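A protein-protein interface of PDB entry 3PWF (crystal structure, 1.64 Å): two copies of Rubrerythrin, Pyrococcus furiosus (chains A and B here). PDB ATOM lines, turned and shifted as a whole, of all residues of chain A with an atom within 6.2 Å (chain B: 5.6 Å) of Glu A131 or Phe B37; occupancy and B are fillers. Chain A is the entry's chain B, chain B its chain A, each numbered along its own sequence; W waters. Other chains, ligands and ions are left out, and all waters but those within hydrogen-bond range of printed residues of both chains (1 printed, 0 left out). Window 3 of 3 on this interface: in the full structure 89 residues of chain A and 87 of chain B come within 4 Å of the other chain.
OG1 of Thr A68 is in hydrogen-bond range of OE2 of Glu B35. The side-chain carboxylate (OD1) of Asp A132 lies within hydrogen-bond range of the backbone NH (N) of Asn B39 (2.8 Å). The side-chain amide nitrogen (ND2) of Asn B39 lies within hydrogen-bond range of the backbone carbonyl oxygen (O) of Ile A133 (2.8 Å). N of Ile B40 sits at hydrogen-bond distance from OD2 of Asp A132 (3.0 Å). N of Pro B38 sits close to OD1 of Asp A132, at 3.4 Å.
O of Ala B32 is in hydrogen-bond range of N of Phe B37 (2.8 Å). The side-chain carboxylate (OE1) of Glu A131 lies within salt-bridge range of the side-chain amino group (NZ) of Lys A126 (3.2 Å).
Among the printed residues, merely in contact across the chains: Thr A68 with Ala B32 (3.3 Å), Glu A131 with Phe B37 (3.5 Å), Thr A68 with Phe B37 (3.6 Å), Asp A132 with Phe B37 (3.7 Å), Ile A133 with Ile B40 (3.9 Å), Thr A68 with Ile B40 (3.9 Å), Ala A127 with Ile B40 (3.9 Å) and Ala A123 with Ile B40 (3.96 Å).
Of the printed residues of chain B, Ala A123 touches Ile B40. Glu A131 touches one residue of chain B. Phe B37 touches just these residues of chain A: Thr A68, Glu A131 and Asp A132. Of the printed residues of chain A, Pro B38 touches Asp A132 (3.3 Å). Of the printed residues of chain A, Asn B39 touches Asp A132 and Ile A133. The nearest residue of chain B that does not touch Glu A131 is Ile B40 (4.4 Å). The nearest residue of chain A that does not touch Phe B37 is Gly A130 (4.1 Å).
Hydrophobic or aromatic side chains of chain A that line the printed part of chain B: Ala A127 and Ile A133. Hydrophobic or aromatic side chains of chain B that line the printed part of chain A: Ala B32, Phe B37, Pro B38 and Ile B40. Along chain B the printed residues that touch a printed residue of chain A span positions 32 to 40. Among the printed residues, no Asp or Glu carboxylate lies within 4 Å of a Lys or Arg side-chain nitrogen of the other chain.
No position is printed for both chains.
Water W1 bridges the side-chain hydroxyl of Thr A68 (3.0 Å) and the backbone NH of Ala B32 (3.4 Å).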
ATOM      1  N   THR A  68     -11.082  22.020  -0.490  1.00  0.00           N
ATOM      2  CA  THR A  68     -10.426  20.686  -0.480  1.00  0.00           C
ATOM      3  C   THR A  68     -10.837  19.696  -1.508  1.00  0.00           C
ATOM      4  O   THR A  68     -10.070  19.085  -2.167  1.00  0.00           O
ATOM      5  CB  THR A  68     -10.337  20.137   0.994  1.00  0.00           C
ATOM      6  OG1 THR A  68      -9.650  21.086   1.823  1.00  0.00           O
ATOM      7  CG2 THR A  68      -9.774  18.757   1.045  1.00  0.00           C
ATOM      8  N   PRO A  69     -12.180  19.488  -1.776  1.00  0.00           N
ATOM      9  CA  PRO A  69     -12.492  18.607  -2.834  1.00  0.00           C
ATOM     10  C   PRO A  69     -12.023  18.998  -4.229  1.00  0.00           C
ATOM     11  O   PRO A  69     -11.580  18.107  -4.980  1.00  0.00           O
ATOM     12  CB  PRO A  69     -14.062  18.607  -2.821  1.00  0.00           C
ATOM     13  CG  PRO A  69     -14.350  18.784  -1.407  1.00  0.00           C
ATOM     14  CD  PRO A  69     -13.383  19.992  -1.091  1.00  0.00           C
ATOM     15  N   ALA A 123      -9.736  10.016  -0.904  1.00  0.00           N
ATOM     16  CA  ALA A 123      -9.951  11.173  -0.123  1.00  0.00           C
ATOM     17  C   ALA A 123     -11.050  12.096  -0.623  1.00  0.00           C
ATOM     18  O   ALA A 123     -11.738  12.666   0.200  1.00  0.00           O
ATOM     19  CB  ALA A 123      -8.576  12.009   0.054  1.00  0.00           C
ATOM     20  N   LYS A 126     -14.489  11.015   0.407  1.00  0.00           N
ATOM     21  CA  LYS A 126     -14.839  11.459   1.813  1.00  0.00           C
ATOM     22  C   LYS A 126     -15.060  12.892   1.918  1.00  0.00           C
ATOM     23  O   LYS A 126     -16.043  13.367   2.470  1.00  0.00           O
ATOM     24  CB  LYS A 126     -13.755  11.051   2.852  1.00  0.00           C
ATOM     25  CG  LYS A 126     -13.532   9.547   2.918  1.00  0.00           C
ATOM     26  CD  LYS A 126     -14.876   8.872   3.339  1.00  0.00           C
ATOM     27  CE  LYS A 126     -14.693   7.520   4.123  1.00  0.00           C
ATOM     28  NZ  LYS A 126     -16.074   7.126   4.658  1.00  0.00           N
ATOM     29  N   ALA A 127     -14.186  13.736   1.290  1.00  0.00           N
ATOM     30  CA  ALA A 127     -14.342  15.152   1.485  1.00  0.00           C
ATOM     31  C   ALA A 127     -15.582  15.712   0.784  1.00  0.00           C
ATOM     32  O   ALA A 127     -16.069  16.715   1.257  1.00  0.00           O
ATOM     33  CB  ALA A 127     -13.078  15.921   0.883  1.00  0.00           C
ATOM     34  N   GLU A 128     -16.055  15.030  -0.245  1.00  0.00           N
ATOM     35  CA  GLU A 128     -17.275  15.437  -1.016  1.00  0.00           C
ATOM     36  C   GLU A 128     -18.442  15.257  -0.021  1.00  0.00           C
ATOM     37  O   GLU A 128     -19.486  15.875  -0.293  1.00  0.00           O
ATOM     38  CB  GLU A 128     -17.633  14.471  -2.190  1.00  0.00           C
ATOM     39  CG  GLU A 128     -16.853  14.495  -3.443  1.00  0.00           C
ATOM     40  CD  GLU A 128     -17.052  15.756  -4.366  1.00  0.00           C
ATOM     41  OE1 GLU A 128     -17.054  16.889  -3.858  1.00  0.00           O
ATOM     42  OE2 GLU A 128     -17.160  15.589  -5.632  1.00  0.00           O
ATOM     43  N   LYS A 129     -18.349  14.352   0.977  1.00  0.00           N
ATOM     44  CA  LYS A 129     -19.493  14.118   1.942  1.00  0.00           C
ATOM     45  C   LYS A 129     -19.267  14.888   3.213  1.00  0.00           C
ATOM     46  O   LYS A 129     -19.922  14.656   4.234  1.00  0.00           O
ATOM     47  CB  LYS A 129     -19.555  12.626   2.268  1.00  0.00           C
ATOM     48  CG  LYS A 129     -20.352  11.899   1.268  1.00  0.00           C
ATOM     49  CD  LYS A 129     -19.928  10.391   1.285  1.00  0.00           C
ATOM     50  CE  LYS A 129     -20.675   9.552   0.181  1.00  0.00           C
ATOM     51  NZ  LYS A 129     -22.199   9.740   0.069  1.00  0.00           N
ATOM     52  N   GLY A 130     -18.255  15.776   3.189  1.00  0.00           N
ATOM     53  CA  GLY A 130     -17.846  16.527   4.372  1.00  0.00           C
ATOM     54  C   GLY A 130     -17.145  15.748   5.458  1.00  0.00           C
ATOM     55  O   GLY A 130     -17.159  16.224   6.615  1.00  0.00           O
ATOM     56  N   GLU A 131     -16.466  14.642   5.121  1.00  0.00           N
ATOM     57  CA  GLU A 131     -15.800  13.830   6.110  1.00  0.00           C
ATOM     58  C   GLU A 131     -14.298  13.933   5.803  1.00  0.00           C
ATOM     59  O   GLU A 131     -13.905  14.063   4.659  1.00  0.00           O
ATOM     60  CB  GLU A 131     -16.196  12.319   6.077  1.00  0.00           C
ATOM     61  CG  GLU A 131     -17.766  12.052   6.419  1.00  0.00           C
ATOM     62  CD  GLU A 131     -18.214  10.663   6.022  1.00  0.00           C
ATOM     63  OE1 GLU A 131     -17.407   9.717   6.092  1.00  0.00           O
ATOM     64  OE2 GLU A 131     -19.366  10.496   5.583  1.00  0.00           O
ATOM     65  N   ASP A 132     -13.532  13.822   6.850  1.00  0.00           N
ATOM     66  CA  ASP A 132     -12.075  13.682   6.706  1.00  0.00           C
ATOM     67  C   ASP A 132     -11.836  12.190   6.426  1.00  0.00           C
ATOM     68  O   ASP A 132     -12.716  11.296   6.590  1.00  0.00           O
ATOM     69  CB  ASP A 132     -11.464  14.061   7.996  1.00  0.00           C
ATOM     70  CG  ASP A 132      -9.920  14.346   7.891  1.00  0.00           C
ATOM     71  OD1 ASP A 132      -9.337  14.564   8.917  1.00  0.00           O
ATOM     72  OD2 ASP A 132      -9.391  14.376   6.741  1.00  0.00           O
ATOM     73  N   ILE A 133     -10.672  11.877   5.885  1.00  0.00           N
ATOM     74  CA  ILE A 133     -10.317  10.459   5.760  1.00  0.00           C
ATOM     75  C   ILE A 133      -9.857   9.930   7.111  1.00  0.00           C
ATOM     76  O   ILE A 133      -9.543  10.685   8.009  1.00  0.00           O
ATOM     77  CB  ILE A 133      -9.186  10.261   4.789  1.00  0.00           C
ATOM     78  CG1 ILE A 133      -7.913  11.024   5.276  1.00  0.00           C
ATOM     79  CG2 ILE A 133      -9.630  10.682   3.470  1.00  0.00           C
ATOM     80  CD1 ILE A 133      -6.736  10.889   4.287  1.00  0.00           C
ATOM     81  N   GLU A 134      -9.887   8.597   7.239  1.00  0.00           N
ATOM     82  CA  GLU A 134      -9.447   7.883   8.396  1.00  0.00           C
ATOM     83  C   GLU A 134      -8.115   7.280   7.949  1.00  0.00           C
ATOM     84  O   GLU A 134      -8.053   6.243   7.266  1.00  0.00           O
ATOM     85  CB  GLU A 134     -10.487   6.764   8.666  1.00  0.00           C
ATOM     86  CG  GLU A 134     -11.854   7.335   9.133  1.00  0.00           C
ATOM     87  CD  GLU A 134     -12.938   6.248   9.398  1.00  0.00           C
ATOM     88  OE1 GLU A 134     -14.063   6.629   9.827  1.00  0.00           O
ATOM     89  OE2 GLU A 134     -12.686   5.026   9.182  1.00  0.00           O
ATOM     90  N   ALA B  32      -6.515  22.450   3.513  1.00  0.00           N
ATOM     91  CA  ALA B  32      -7.255  21.359   4.139  1.00  0.00           C
ATOM     92  C   ALA B  32      -7.258  21.517   5.699  1.00  0.00           C
ATOM     93  O   ALA B  32      -8.319  21.218   6.348  1.00  0.00           O
ATOM     94  CB  ALA B  32      -6.594  20.016   3.759  1.00  0.00           C
ATOM     95  N   GLU B  33      -6.133  21.925   6.268  1.00  0.00           N
ATOM     96  CA  GLU B  33      -6.030  22.156   7.742  1.00  0.00           C
ATOM     97  C   GLU B  33      -7.052  23.257   8.115  1.00  0.00           C
ATOM     98  O   GLU B  33      -7.885  23.026   9.037  1.00  0.00           O
ATOM     99  CB  GLU B  33      -4.564  22.552   8.127  1.00  0.00           C
ATOM    100  CG  GLU B  33      -4.313  22.428   9.648  1.00  0.00           C
ATOM    101  CD  GLU B  33      -4.151  20.949  10.146  1.00  0.00           C
ATOM    102  OE1 GLU B  33      -3.318  20.128   9.628  1.00  0.00           O
ATOM    103  OE2 GLU B  33      -4.857  20.649  11.139  1.00  0.00           O
ATOM    104  N   GLU B  35      -9.732  24.135   6.629  1.00  0.00           N
ATOM    105  CA  GLU B  35     -11.130  23.737   6.416  1.00  0.00           C
ATOM    106  C   GLU B  35     -11.604  22.608   7.361  1.00  0.00           C
ATOM    107  O   GLU B  35     -12.796  22.181   7.277  1.00  0.00           O
ATOM    108  CB  GLU B  35     -11.378  23.316   4.969  1.00  0.00           C
ATOM    109  CG  GLU B  35     -11.336  24.492   4.014  1.00  0.00           C
ATOM    110  CD  GLU B  35     -11.706  24.062   2.604  1.00  0.00           C
ATOM    111  OE1 GLU B  35     -12.410  24.827   1.843  1.00  0.00           O
ATOM    112  OE2 GLU B  35     -11.361  22.961   2.201  1.00  0.00           O
ATOM    113  N   GLY B  36     -10.696  22.071   8.162  1.00  0.00           N
ATOM    114  CA  GLY B  36     -11.126  20.972   9.167  1.00  0.00           C
ATOM    115  C   GLY B  36     -10.951  19.570   8.694  1.00  0.00           C
ATOM    116  O   GLY B  36     -11.550  18.612   9.252  1.00  0.00           O
ATOM    117  N   PHE B  37      -9.987  19.388   7.733  1.00  0.00           N
ATOM    118  CA  PHE B  37      -9.627  18.052   7.270  1.00  0.00           C
ATOM    119  C   PHE B  37      -8.139  17.775   7.646  1.00  0.00           C
ATOM    120  O   PHE B  37      -7.293  17.627   6.735  1.00  0.00           O
ATOM    121  CB  PHE B  37      -9.802  17.905   5.748  1.00  0.00           C
ATOM    122  CG  PHE B  37     -11.202  18.239   5.230  1.00  0.00           C
ATOM    123  CD1 PHE B  37     -11.429  19.446   4.552  1.00  0.00           C
ATOM    124  CD2 PHE B  37     -12.202  17.267   5.309  1.00  0.00           C
ATOM    125  CE1 PHE B  37     -12.733  19.687   4.009  1.00  0.00           C
ATOM    126  CE2 PHE B  37     -13.523  17.543   4.779  1.00  0.00           C
ATOM    127  CZ  PHE B  37     -13.735  18.700   4.133  1.00  0.00           C
ATOM    128  N   PRO B  38      -7.829  17.557   8.921  1.00  0.00           N
ATOM    129  CA  PRO B  38      -6.423  17.294   9.309  1.00  0.00           C
ATOM    130  C   PRO B  38      -5.826  16.068   8.711  1.00  0.00           C
ATOM    131  O   PRO B  38      -4.573  16.108   8.427  1.00  0.00           O
ATOM    132  CB  PRO B  38      -6.447  17.195  10.870  1.00  0.00           C
ATOM    133  CG  PRO B  38      -7.918  16.797  11.159  1.00  0.00           C
ATOM    134  CD  PRO B  38      -8.718  17.588  10.126  1.00  0.00           C
ATOM    135  N   ASN B  39      -6.585  15.002   8.514  1.00  0.00           N
ATOM    136  CA  ASN B  39      -5.921  13.803   8.025  1.00  0.00           C
ATOM    137  C   ASN B  39      -5.651  13.974   6.509  1.00  0.00           C
ATOM    138  O   ASN B  39      -4.647  13.448   6.026  1.00  0.00           O
ATOM    139  CB  ASN B  39      -6.734  12.517   8.274  1.00  0.00           C
ATOM    140  CG  ASN B  39      -6.800  12.206   9.720  1.00  0.00           C
ATOM    141  OD1 ASN B  39      -5.871  12.551  10.454  1.00  0.00           O
ATOM    142  ND2 ASN B  39      -7.878  11.495  10.152  1.00  0.00           N
ATOM    143  N   ILE B  40      -6.572  14.612   5.765  1.00  0.00           N
ATOM    144  CA  ILE B  40      -6.278  14.949   4.318  1.00  0.00           C
ATOM    145  C   ILE B  40      -5.036  15.891   4.256  1.00  0.00           C
ATOM    146  O   ILE B  40      -4.206  15.767   3.333  1.00  0.00           O
ATOM    147  CB  ILE B  40      -7.474  15.553   3.625  1.00  0.00           C
ATOM    148  CG1 ILE B  40      -8.512  14.390   3.404  1.00  0.00           C
ATOM    149  CG2 ILE B  40      -7.131  16.169   2.203  1.00  0.00           C
ATOM    150  CD1 ILE B  40      -9.944  14.847   2.975  1.00  0.00           C
ATOM    151  N   ALA B  41      -4.963  16.829   5.196  1.00  0.00           N
ATOM    152  CA  ALA B  41      -3.758  17.718   5.167  1.00  0.00           C
ATOM    153  C   ALA B  41      -2.544  16.882   5.370  1.00  0.00           C
ATOM    154  O   ALA B  41      -1.513  17.184   4.696  1.00  0.00           O
ATOM    155  CB  ALA B  41      -3.806  18.748   6.295  1.00  0.00           C
ATOM    156  N   LYS B  42      -2.591  15.882   6.304  1.00  0.00           N
ATOM    157  CA  LYS B  42      -1.381  15.026   6.524  1.00  0.00           C
ATOM    158  C   LYS B  42      -1.009  14.253   5.243  1.00  0.00           C
ATOM    159  O   LYS B  42       0.140  14.100   4.924  1.00  0.00           O
ATOM    160  CB  LYS B  42      -1.741  14.037   7.714  1.00  0.00           C
ATOM    161  CG  LYS B  42      -0.557  13.057   8.010  1.00  0.00           C
ATOM    162  CD  LYS B  42      -0.888  12.031   9.163  1.00  0.00           C
ATOM    163  CE  LYS B  42      -1.912  12.530  10.121  1.00  0.00           C
ATOM    164  NZ  LYS B  42      -1.854  11.636  11.419  1.00  0.00           N
HETATM  165  O   HOH W   1      -7.104  21.439   0.346  1.00  0.00           O
